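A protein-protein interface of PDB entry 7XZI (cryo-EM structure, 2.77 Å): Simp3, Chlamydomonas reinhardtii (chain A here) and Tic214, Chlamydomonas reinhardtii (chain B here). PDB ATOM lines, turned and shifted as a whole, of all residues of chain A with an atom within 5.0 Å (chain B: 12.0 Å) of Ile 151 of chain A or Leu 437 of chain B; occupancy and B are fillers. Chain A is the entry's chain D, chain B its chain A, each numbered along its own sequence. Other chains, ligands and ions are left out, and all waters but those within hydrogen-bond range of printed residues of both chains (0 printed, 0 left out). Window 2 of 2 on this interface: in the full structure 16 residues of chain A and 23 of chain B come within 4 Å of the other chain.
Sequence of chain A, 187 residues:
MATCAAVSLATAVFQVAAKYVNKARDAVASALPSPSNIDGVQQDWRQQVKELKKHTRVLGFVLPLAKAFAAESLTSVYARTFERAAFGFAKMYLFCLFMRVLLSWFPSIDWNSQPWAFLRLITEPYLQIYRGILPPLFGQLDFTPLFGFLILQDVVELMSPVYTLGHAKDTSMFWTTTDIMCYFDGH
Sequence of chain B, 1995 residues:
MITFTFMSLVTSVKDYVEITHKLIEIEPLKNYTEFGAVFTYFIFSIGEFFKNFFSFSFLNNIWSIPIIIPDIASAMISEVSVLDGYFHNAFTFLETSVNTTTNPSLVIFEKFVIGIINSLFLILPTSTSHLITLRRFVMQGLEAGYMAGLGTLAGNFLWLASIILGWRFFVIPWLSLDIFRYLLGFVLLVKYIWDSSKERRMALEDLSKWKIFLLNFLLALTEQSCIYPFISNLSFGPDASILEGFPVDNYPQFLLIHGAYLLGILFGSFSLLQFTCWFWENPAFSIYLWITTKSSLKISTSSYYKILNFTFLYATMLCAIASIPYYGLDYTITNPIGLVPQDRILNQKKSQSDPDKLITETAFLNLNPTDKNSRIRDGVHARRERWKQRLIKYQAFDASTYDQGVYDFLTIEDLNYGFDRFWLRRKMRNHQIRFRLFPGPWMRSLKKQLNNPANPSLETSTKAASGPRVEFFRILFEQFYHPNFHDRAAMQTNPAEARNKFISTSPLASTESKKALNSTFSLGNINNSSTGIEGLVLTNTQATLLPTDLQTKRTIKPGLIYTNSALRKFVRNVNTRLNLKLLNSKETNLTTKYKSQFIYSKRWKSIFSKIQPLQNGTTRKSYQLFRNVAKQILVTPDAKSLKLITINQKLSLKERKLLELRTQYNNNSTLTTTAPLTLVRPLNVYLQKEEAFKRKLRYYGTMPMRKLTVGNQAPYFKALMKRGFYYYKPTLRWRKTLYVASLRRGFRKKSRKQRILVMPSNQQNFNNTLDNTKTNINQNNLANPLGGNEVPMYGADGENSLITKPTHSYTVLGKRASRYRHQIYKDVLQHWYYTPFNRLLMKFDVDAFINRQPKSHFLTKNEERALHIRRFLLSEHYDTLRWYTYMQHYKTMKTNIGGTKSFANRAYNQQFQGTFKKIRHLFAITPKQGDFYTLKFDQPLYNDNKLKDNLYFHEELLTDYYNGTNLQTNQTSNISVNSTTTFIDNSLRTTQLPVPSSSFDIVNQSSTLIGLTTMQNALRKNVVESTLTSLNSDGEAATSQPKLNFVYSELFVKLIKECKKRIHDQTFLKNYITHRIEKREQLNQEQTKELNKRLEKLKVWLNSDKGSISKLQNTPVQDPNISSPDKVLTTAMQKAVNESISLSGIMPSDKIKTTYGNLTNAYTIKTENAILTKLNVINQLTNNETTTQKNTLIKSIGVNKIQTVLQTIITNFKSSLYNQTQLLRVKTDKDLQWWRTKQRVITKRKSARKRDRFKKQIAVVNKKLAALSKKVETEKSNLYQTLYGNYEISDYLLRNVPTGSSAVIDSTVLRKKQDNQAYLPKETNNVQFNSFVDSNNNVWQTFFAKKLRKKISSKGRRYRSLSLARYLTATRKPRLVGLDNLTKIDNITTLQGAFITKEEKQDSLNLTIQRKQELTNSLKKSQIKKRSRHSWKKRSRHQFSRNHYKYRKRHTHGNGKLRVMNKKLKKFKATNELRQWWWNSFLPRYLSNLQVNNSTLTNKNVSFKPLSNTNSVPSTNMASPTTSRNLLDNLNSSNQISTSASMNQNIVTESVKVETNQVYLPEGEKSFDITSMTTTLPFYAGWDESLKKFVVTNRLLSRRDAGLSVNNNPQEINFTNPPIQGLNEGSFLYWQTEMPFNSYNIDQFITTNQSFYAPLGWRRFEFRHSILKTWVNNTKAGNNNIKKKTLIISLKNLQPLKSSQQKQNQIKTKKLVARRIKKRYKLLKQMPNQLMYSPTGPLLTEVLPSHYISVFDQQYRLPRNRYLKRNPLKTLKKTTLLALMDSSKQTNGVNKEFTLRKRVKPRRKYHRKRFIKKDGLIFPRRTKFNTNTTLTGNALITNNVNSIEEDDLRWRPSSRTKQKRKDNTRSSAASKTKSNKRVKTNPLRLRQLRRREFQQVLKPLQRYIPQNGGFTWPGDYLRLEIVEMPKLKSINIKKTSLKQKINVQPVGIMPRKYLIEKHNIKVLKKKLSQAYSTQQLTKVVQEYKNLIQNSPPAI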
ATOM      1  N   TYR A 126       5.207  19.312 -14.851  1.00  0.00           N
ATOM      2  CA  TYR A 126       4.541  20.155 -15.838  1.00  0.00           C
ATOM      3  C   TYR A 126       3.161  20.587 -15.358  1.00  0.00           C
ATOM      4  O   TYR A 126       2.782  21.756 -15.503  1.00  0.00           O
ATOM      5  CB  TYR A 126       4.441  19.417 -17.173  1.00  0.00           C
ATOM      6  CG  TYR A 126       3.729  20.197 -18.253  1.00  0.00           C
ATOM      7  CD1 TYR A 126       4.377  21.208 -18.949  1.00  0.00           C
ATOM      8  CD2 TYR A 126       2.410  19.918 -18.584  1.00  0.00           C
ATOM      9  CE1 TYR A 126       3.730  21.922 -19.938  1.00  0.00           C
ATOM     10  CE2 TYR A 126       1.756  20.626 -19.571  1.00  0.00           C
ATOM     11  CZ  TYR A 126       2.420  21.626 -20.246  1.00  0.00           C
ATOM     12  OH  TYR A 126       1.771  22.332 -21.230  1.00  0.00           O
ATOM     13  N   TYR A 130       1.369  24.461 -13.619  1.00  0.00           N
ATOM     14  CA  TYR A 130       0.069  25.052 -13.921  1.00  0.00           C
ATOM     15  C   TYR A 130      -0.847  25.074 -12.704  1.00  0.00           C
ATOM     16  O   TYR A 130      -1.737  25.927 -12.622  1.00  0.00           O
ATOM     17  CB  TYR A 130      -0.591  24.309 -15.081  1.00  0.00           C
ATOM     18  CG  TYR A 130      -0.258  24.902 -16.431  1.00  0.00           C
ATOM     19  CD1 TYR A 130       0.885  24.517 -17.119  1.00  0.00           C
ATOM     20  CD2 TYR A 130      -1.081  25.858 -17.008  1.00  0.00           C
ATOM     21  CE1 TYR A 130       1.193  25.063 -18.350  1.00  0.00           C
ATOM     22  CE2 TYR A 130      -0.782  26.408 -18.237  1.00  0.00           C
ATOM     23  CZ  TYR A 130       0.356  26.008 -18.904  1.00  0.00           C
ATOM     24  OH  TYR A 130       0.655  26.558 -20.127  1.00  0.00           O
ATOM     25  N   LEU A 146      -6.355  19.359 -18.086  1.00  0.00           N
ATOM     26  CA  LEU A 146      -6.905  19.696 -19.396  1.00  0.00           C
ATOM     27  C   LEU A 146      -6.211  20.914 -19.992  1.00  0.00           C
ATOM     28  O   LEU A 146      -5.888  20.929 -21.186  1.00  0.00           O
ATOM     29  CB  LEU A 146      -8.412  19.931 -19.287  1.00  0.00           C
ATOM     30  CG  LEU A 146      -9.149  20.302 -20.575  1.00  0.00           C
ATOM     31  CD1 LEU A 146      -9.027  19.192 -21.606  1.00  0.00           C
ATOM     32  CD2 LEU A 146     -10.611  20.614 -20.288  1.00  0.00           C
ATOM     33  N   PHE A 147      -5.972  21.944 -19.177  1.00  0.00           N
ATOM     34  CA  PHE A 147      -5.271  23.127 -19.666  1.00  0.00           C
ATOM     35  C   PHE A 147      -3.845  22.794 -20.080  1.00  0.00           C
ATOM     36  O   PHE A 147      -3.368  23.258 -21.123  1.00  0.00           O
ATOM     37  CB  PHE A 147      -5.281  24.222 -18.600  1.00  0.00           C
ATOM     38  CG  PHE A 147      -6.505  25.089 -18.635  1.00  0.00           C
ATOM     39  CD1 PHE A 147      -7.673  24.692 -18.005  1.00  0.00           C
ATOM     40  CD2 PHE A 147      -6.487  26.303 -19.299  1.00  0.00           C
ATOM     41  CE1 PHE A 147      -8.801  25.491 -18.038  1.00  0.00           C
ATOM     42  CE2 PHE A 147      -7.611  27.105 -19.336  1.00  0.00           C
ATOM     43  CZ  PHE A 147      -8.769  26.699 -18.704  1.00  0.00           C
ATOM     44  N   GLY A 148      -3.145  21.993 -19.273  1.00  0.00           N
ATOM     45  CA  GLY A 148      -1.804  21.578 -19.650  1.00  0.00           C
ATOM     46  C   GLY A 148      -1.785  20.791 -20.946  1.00  0.00           C
ATOM     47  O   GLY A 148      -0.927  21.011 -21.807  1.00  0.00           O
ATOM     48  N   PHE A 149      -2.739  19.871 -21.107  1.00  0.00           N
ATOM     49  CA  PHE A 149      -2.831  19.083 -22.330  1.00  0.00           C
ATOM     50  C   PHE A 149      -3.089  19.974 -23.538  1.00  0.00           C
ATOM     51  O   PHE A 149      -2.471  19.798 -24.592  1.00  0.00           O
ATOM     52  CB  PHE A 149      -3.930  18.028 -22.183  1.00  0.00           C
ATOM     53  CG  PHE A 149      -4.338  17.383 -23.479  1.00  0.00           C
ATOM     54  CD1 PHE A 149      -3.598  16.342 -24.016  1.00  0.00           C
ATOM     55  CD2 PHE A 149      -5.475  17.804 -24.149  1.00  0.00           C
ATOM     56  CE1 PHE A 149      -3.979  15.744 -25.204  1.00  0.00           C
ATOM     57  CE2 PHE A 149      -5.860  17.210 -25.336  1.00  0.00           C
ATOM     58  CZ  PHE A 149      -5.111  16.179 -25.864  1.00  0.00           C
ATOM     59  N   LEU A 150      -4.001  20.939 -23.403  1.00  0.00           N
ATOM     60  CA  LEU A 150      -4.301  21.831 -24.521  1.00  0.00           C
ATOM     61  C   LEU A 150      -3.098  22.691 -24.887  1.00  0.00           C
ATOM     62  O   LEU A 150      -2.787  22.868 -26.074  1.00  0.00           O
ATOM     63  CB  LEU A 150      -5.505  22.710 -24.182  1.00  0.00           C
ATOM     64  CG  LEU A 150      -6.857  22.006 -24.063  1.00  0.00           C
ATOM     65  CD1 LEU A 150      -7.945  22.995 -23.673  1.00  0.00           C
ATOM     66  CD2 LEU A 150      -7.206  21.306 -25.365  1.00  0.00           C
ATOM     67  N   ILE A 151      -2.409  23.237 -23.882  1.00  0.00           N
ATOM     68  CA  ILE A 151      -1.245  24.077 -24.154  1.00  0.00           C
ATOM     69  C   ILE A 151      -0.149  23.265 -24.834  1.00  0.00           C
ATOM     70  O   ILE A 151       0.456  23.714 -25.816  1.00  0.00           O
ATOM     71  CB  ILE A 151      -0.746  24.747 -22.858  1.00  0.00           C
ATOM     72  CG1 ILE A 151      -1.397  26.122 -22.670  1.00  0.00           C
ATOM     73  CG2 ILE A 151       0.770  24.891 -22.870  1.00  0.00           C
ATOM     74  CD1 ILE A 151      -2.897  26.091 -22.473  1.00  0.00           C
ATOM     75  N   LEU A 152       0.115  22.053 -24.337  1.00  0.00           N
ATOM     76  CA  LEU A 152       1.141  21.225 -24.961  1.00  0.00           C
ATOM     77  C   LEU A 152       0.733  20.792 -26.364  1.00  0.00           C
ATOM     78  O   LEU A 152       1.590  20.685 -27.249  1.00  0.00           O
ATOM     79  CB  LEU A 152       1.443  20.003 -24.095  1.00  0.00           C
ATOM     80  CG  LEU A 152       2.632  19.169 -24.575  1.00  0.00           C
ATOM     81  CD1 LEU A 152       3.883  20.031 -24.649  1.00  0.00           C
ATOM     82  CD2 LEU A 152       2.861  17.969 -23.677  1.00  0.00           C
ATOM     83  N   GLN A 153      -0.559  20.545 -26.589  1.00  0.00           N
ATOM     84  CA  GLN A 153      -1.034  20.206 -27.925  1.00  0.00           C
ATOM     85  C   GLN A 153      -0.797  21.355 -28.895  1.00  0.00           C
ATOM     86  O   GLN A 153      -0.331  21.147 -30.020  1.00  0.00           O
ATOM     87  CB  GLN A 153      -2.517  19.838 -27.872  1.00  0.00           C
ATOM     88  CG  GLN A 153      -3.201  19.801 -29.228  1.00  0.00           C
ATOM     89  CD  GLN A 153      -4.681  19.495 -29.121  1.00  0.00           C
ATOM     90  OE1 GLN A 153      -5.500  20.073 -29.837  1.00  0.00           O
ATOM     91  NE2 GLN A 153      -5.033  18.580 -28.226  1.00  0.00           N
ATOM     92  N   ASP A 154      -1.100  22.584 -28.472  1.00  0.00           N
ATOM     93  CA  ASP A 154      -0.832  23.734 -29.332  1.00  0.00           C
ATOM     94  C   ASP A 154       0.663  23.898 -29.585  1.00  0.00           C
ATOM     95  O   ASP A 154       1.084  24.175 -30.717  1.00  0.00           O
ATOM     96  CB  ASP A 154      -1.418  25.005 -28.715  1.00  0.00           C
ATOM     97  CG  ASP A 154      -2.927  25.084 -28.862  1.00  0.00           C
ATOM     98  OD1 ASP A 154      -3.523  24.144 -29.429  1.00  0.00           O
ATOM     99  OD2 ASP A 154      -3.515  26.089 -28.413  1.00  0.00           O
ATOM    100  N   VAL A 155       1.482  23.716 -28.546  1.00  0.00           N
ATOM    101  CA  VAL A 155       2.926  23.883 -28.697  1.00  0.00           C
ATOM    102  C   VAL A 155       3.486  22.865 -29.683  1.00  0.00           C
ATOM    103  O   VAL A 155       4.286  23.207 -30.561  1.00  0.00           O
ATOM    104  CB  VAL A 155       3.621  23.789 -27.324  1.00  0.00           C
ATOM    105  CG1 VAL A 155       5.127  23.675 -27.494  1.00  0.00           C
ATOM    106  CG2 VAL A 155       3.277  25.003 -26.477  1.00  0.00           C
ATOM    107  N   ILE B 433      -4.271  22.258 -40.009  1.00  0.00           N
ATOM    108  CA  ILE B 433      -3.681  23.066 -38.947  1.00  0.00           C
ATOM    109  C   ILE B 433      -4.807  23.683 -38.130  1.00  0.00           C
ATOM    110  O   ILE B 433      -5.694  24.346 -38.683  1.00  0.00           O
ATOM    111  CB  ILE B 433      -2.756  24.151 -39.523  1.00  0.00           C
ATOM    112  CG1 ILE B 433      -1.776  23.542 -40.528  1.00  0.00           C
ATOM    113  CG2 ILE B 433      -2.007  24.862 -38.407  1.00  0.00           C
ATOM    114  CD1 ILE B 433      -0.861  22.490 -39.939  1.00  0.00           C
ATOM    115  N   ARG B 434      -4.775  23.469 -36.817  1.00  0.00           N
ATOM    116  CA  ARG B 434      -5.818  23.972 -35.935  1.00  0.00           C
ATOM    117  C   ARG B 434      -5.211  24.333 -34.588  1.00  0.00           C
ATOM    118  O   ARG B 434      -4.313  23.643 -34.097  1.00  0.00           O
ATOM    119  CB  ARG B 434      -6.940  22.943 -35.755  1.00  0.00           C
ATOM    120  CG  ARG B 434      -6.468  21.593 -35.239  1.00  0.00           C
ATOM    121  CD  ARG B 434      -7.610  20.596 -35.156  1.00  0.00           C
ATOM    122  NE  ARG B 434      -8.186  20.321 -36.464  1.00  0.00           N
ATOM    123  CZ  ARG B 434      -7.732  19.398 -37.304  1.00  0.00           C
ATOM    124  NH1 ARG B 434      -6.685  18.646 -37.006  1.00  0.00           N
ATOM    125  NH2 ARG B 434      -8.344  19.225 -38.471  1.00  0.00           N
ATOM    126  N   PHE B 435      -5.704  25.421 -34.000  1.00  0.00           N
ATOM    127  CA  PHE B 435      -5.288  25.873 -32.675  1.00  0.00           C
ATOM    128  C   PHE B 435      -6.539  26.021 -31.818  1.00  0.00           C
ATOM    129  O   PHE B 435      -7.406  26.850 -32.116  1.00  0.00           O
ATOM    130  CB  PHE B 435      -4.509  27.184 -32.763  1.00  0.00           C
ATOM    131  CG  PHE B 435      -3.307  27.110 -33.660  1.00  0.00           C
ATOM    132  CD1 PHE B 435      -2.105  26.608 -33.188  1.00  0.00           C
ATOM    133  CD2 PHE B 435      -3.382  27.531 -34.976  1.00  0.00           C
ATOM    134  CE1 PHE B 435      -0.998  26.534 -34.012  1.00  0.00           C
ATOM    135  CE2 PHE B 435      -2.279  27.460 -35.805  1.00  0.00           C
ATOM    136  CZ  PHE B 435      -1.086  26.960 -35.323  1.00  0.00           C
ATOM    137  N   ARG B 436      -6.632  25.217 -30.757  1.00  0.00           N
ATOM    138  CA  ARG B 436      -7.867  25.157 -29.983  1.00  0.00           C
ATOM    139  C   ARG B 436      -8.044  26.382 -29.093  1.00  0.00           C
ATOM    140  O   ARG B 436      -9.164  26.882 -28.938  1.00  0.00           O
ATOM    141  CB  ARG B 436      -7.898  23.876 -29.149  1.00  0.00           C
ATOM    142  CG  ARG B 436      -8.026  22.609 -29.978  1.00  0.00           C
ATOM    143  CD  ARG B 436      -9.263  22.659 -30.861  1.00  0.00           C
ATOM    144  NE  ARG B 436      -9.397  21.467 -31.686  1.00  0.00           N
ATOM    145  CZ  ARG B 436     -10.375  21.270 -32.563  1.00  0.00           C
ATOM    146  NH1 ARG B 436     -11.326  22.170 -32.754  1.00  0.00           N
ATOM    147  NH2 ARG B 436     -10.399  20.141 -33.265  1.00  0.00           N
ATOM    148  N   LEU B 437      -6.961  26.882 -28.501  1.00  0.00           N
ATOM    149  CA  LEU B 437      -7.039  27.986 -27.551  1.00  0.00           C
ATOM    150  C   LEU B 437      -6.446  29.279 -28.085  1.00  0.00           C
ATOM    151  O   LEU B 437      -7.117  30.317 -28.075  1.00  0.00           O
ATOM    152  CB  LEU B 437      -6.341  27.602 -26.238  1.00  0.00           C
ATOM    153  CG  LEU B 437      -7.000  26.504 -25.401  1.00  0.00           C
ATOM    154  CD1 LEU B 437      -6.233  26.289 -24.108  1.00  0.00           C
ATOM    155  CD2 LEU B 437      -8.454  26.844 -25.115  1.00  0.00           C
ATOM    156  N   PHE B 438      -5.200  29.251 -28.547  1.00  0.00           N
ATOM    157  CA  PHE B 438      -4.544  30.469 -28.990  1.00  0.00           C
ATOM    158  C   PHE B 438      -5.185  30.990 -30.276  1.00  0.00           C
ATOM    159  O   PHE B 438      -5.715  30.212 -31.076  1.00  0.00           O
ATOM    160  CB  PHE B 438      -3.054  30.219 -29.210  1.00  0.00           C
ATOM    161  CG  PHE B 438      -2.303  29.899 -27.949  1.00  0.00           C
ATOM    162  CD1 PHE B 438      -2.772  30.333 -26.719  1.00  0.00           C
ATOM    163  CD2 PHE B 438      -1.130  29.164 -27.991  1.00  0.00           C
ATOM    164  CE1 PHE B 438      -2.085  30.041 -25.557  1.00  0.00           C
ATOM    165  CE2 PHE B 438      -0.439  28.868 -26.831  1.00  0.00           C
ATOM    166  CZ  PHE B 438      -0.917  29.307 -25.612  1.00  0.00           C
ATOM    167  N   PRO B 439      -5.167  32.306 -30.489  1.00  0.00           N
ATOM    168  CA  PRO B 439      -5.764  32.862 -31.710  1.00  0.00           C
ATOM    169  C   PRO B 439      -5.038  32.389 -32.961  1.00  0.00           C
ATOM    170  O   PRO B 439      -3.829  32.146 -32.955  1.00  0.00           O
ATOM    171  CB  PRO B 439      -5.624  34.378 -31.517  1.00  0.00           C
ATOM    172  CG  PRO B 439      -4.523  34.537 -30.520  1.00  0.00           C
ATOM    173  CD  PRO B 439      -4.640  33.358 -29.605  1.00  0.00           C
ATOM    174  N   GLY B 440      -5.802  32.262 -34.042  1.00  0.00           N
ATOM    175  CA  GLY B 440      -5.302  31.752 -35.297  1.00  0.00           C
ATOM    176  C   GLY B 440      -4.195  32.565 -35.945  1.00  0.00           C
ATOM    177  O   GLY B 440      -3.119  32.036 -36.245  1.00  0.00           O
ATOM    178  N   PRO B 441      -4.443  33.856 -36.208  1.00  0.00           N
ATOM    179  CA  PRO B 441      -3.436  34.650 -36.937  1.00  0.00           C
ATOM    180  C   PRO B 441      -2.082  34.724 -36.252  1.00  0.00           C
ATOM    181  O   PRO B 441      -1.052  34.664 -36.934  1.00  0.00           O
ATOM    182  CB  PRO B 441      -4.095  36.034 -37.045  1.00  0.00           C
ATOM    183  CG  PRO B 441      -5.166  36.043 -36.003  1.00  0.00           C
ATOM    184  CD  PRO B 441      -5.663  34.638 -35.950  1.00  0.00           C
ATOM    185  N   TRP B 442      -2.046  34.843 -34.923  1.00  0.00           N
ATOM    186  CA  TRP B 442      -0.764  34.950 -34.230  1.00  0.00           C
ATOM    187  C   TRP B 442       0.037  33.659 -34.356  1.00  0.00           C
ATOM    188  O   TRP B 442       1.239  33.687 -34.651  1.00  0.00           O
ATOM    189  CB  TRP B 442      -0.991  35.302 -32.759  1.00  0.00           C
ATOM    190  CG  TRP B 442       0.278  35.540 -31.996  1.00  0.00           C
ATOM    191  CD1 TRP B 442       1.485  35.920 -32.510  1.00  0.00           C
ATOM    192  CD2 TRP B 442       0.471  35.403 -30.583  1.00  0.00           C
ATOM    193  NE1 TRP B 442       2.414  36.034 -31.505  1.00  0.00           N
ATOM    194  CE2 TRP B 442       1.817  35.721 -30.311  1.00  0.00           C
ATOM    195  CE3 TRP B 442      -0.365  35.045 -29.521  1.00  0.00           C
ATOM    196  CZ2 TRP B 442       2.346  35.691 -29.023  1.00  0.00           C
ATOM    197  CZ3 TRP B 442       0.163  35.016 -28.242  1.00  0.00           C
ATOM    198  CH2 TRP B 442       1.504  35.337 -28.004  1.00  0.00           C
ATOM    199  N   MET B 443      -0.616  32.517 -34.140  1.00  0.00           N
ATOM    200  CA  MET B 443       0.071  31.236 -34.271  1.00  0.00           C
ATOM    201  C   MET B 443       0.506  30.992 -35.709  1.00  0.00           C
ATOM    202  O   MET B 443       1.589  30.448 -35.953  1.00  0.00           O
ATOM    203  CB  MET B 443      -0.830  30.105 -33.777  1.00  0.00           C
ATOM    204  CG  MET B 443      -1.262  30.246 -32.329  1.00  0.00           C
ATOM    205  SD  MET B 443       0.129  30.386 -31.188  1.00  0.00           S
ATOM    206  CE  MET B 443       0.947  28.815 -31.452  1.00  0.00           C
ATOM    207  N   ARG B 444      -0.330  31.380 -36.676  1.00  0.00           N
ATOM    208  CA  ARG B 444       0.047  31.233 -38.079  1.00  0.00           C
ATOM    209  C   ARG B 444       1.269  32.076 -38.416  1.00  0.00           C
ATOM    210  O   ARG B 444       2.178  31.613 -39.113  1.00  0.00           O
ATOM    211  CB  ARG B 444      -1.130  31.608 -38.979  1.00  0.00           C
ATOM    212  CG  ARG B 444      -2.182  30.522 -39.106  1.00  0.00           C
ATOM    213  CD  ARG B 444      -1.595  29.279 -39.748  1.00  0.00           C
ATOM    214  NE  ARG B 444      -0.964  29.580 -41.025  1.00  0.00           N
ATOM    215  CZ  ARG B 444      -0.345  28.684 -41.787  1.00  0.00           C
ATOM    216  NH1 ARG B 444      -0.257  27.414 -41.429  1.00  0.00           N
ATOM    217  NH2 ARG B 444       0.198  29.073 -42.936  1.00  0.00           N
ATOM    218  N   LEU B 446       3.591  33.089 -36.293  1.00  0.00           N
ATOM    219  CA  LEU B 446       4.744  32.500 -35.619  1.00  0.00           C
ATOM    220  C   LEU B 446       5.249  31.271 -36.366  1.00  0.00           C
ATOM    221  O   LEU B 446       6.462  31.079 -36.513  1.00  0.00           O
ATOM    222  CB  LEU B 446       4.383  32.151 -34.174  1.00  0.00           C
ATOM    223  CG  LEU B 446       5.501  32.176 -33.124  1.00  0.00           C
ATOM    224  CD1 LEU B 446       4.908  32.271 -31.727  1.00  0.00           C
ATOM    225  CD2 LEU B 446       6.405  30.955 -33.229  1.00  0.00           C
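Tyr 126 of chain A touches none of the printed residues of chain B.
No residue of chain B comes within 4 Å of Phe 147 of chain A.
No residue of chain B comes within 4 Å of Gly 148 of chain A.
Of chain B, only Leu 437 (3.7 Å) comes within 4 Å of Ile 151 of chain A.
Asp 154 of chain A touches three residues of chain B.
Val 155 of chain A touches none of the printed residues of chain B.
Of the printed residues of chain A, Arg 436 of chain B touches Gln 153 and Asp 154.
Of chain A, only Leu 150 (3.7 Å), Ile 151 (3.7 Å) and Asp 154 (3.5 Å) come within 4 Å of Leu 437 of chain B.
Of the printed residues of chain A, Phe 438 of chain B touches Asp 154.
Pro 441 of chain B touches none of the printed residues of chain A.
The nearest residue of chain A that does not touch Leu 437 of chain B is Phe 147 of chain A (4.8 Å).
Leu 150 of chain A touches Leu 437 of chain B.
CD1 of Ile 151 of chain A touches CD1 of Leu 437 of chain B, at 3.7 Å.
Arg 436 of chain B touches Gln 153 of chain A (CG to OE1, 3.6 Å).
Asp 154 of chain A touches Arg 436 of chain B (OD1 to N, 3.5 Å).
Asp 154 of chain A touches Leu 437 of chain B (OD2 to N, 3.5 Å).
N of Phe 438 of chain B touches OD2 of Asp 154 of chain A, at 3.6 Å.
Hydrophobic or aromatic side chains of chain A that line the printed part of chain B: Leu 150 and Ile 151.
Along chain A the printed residues that touch a printed residue of chain B span positions 150 to 154.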
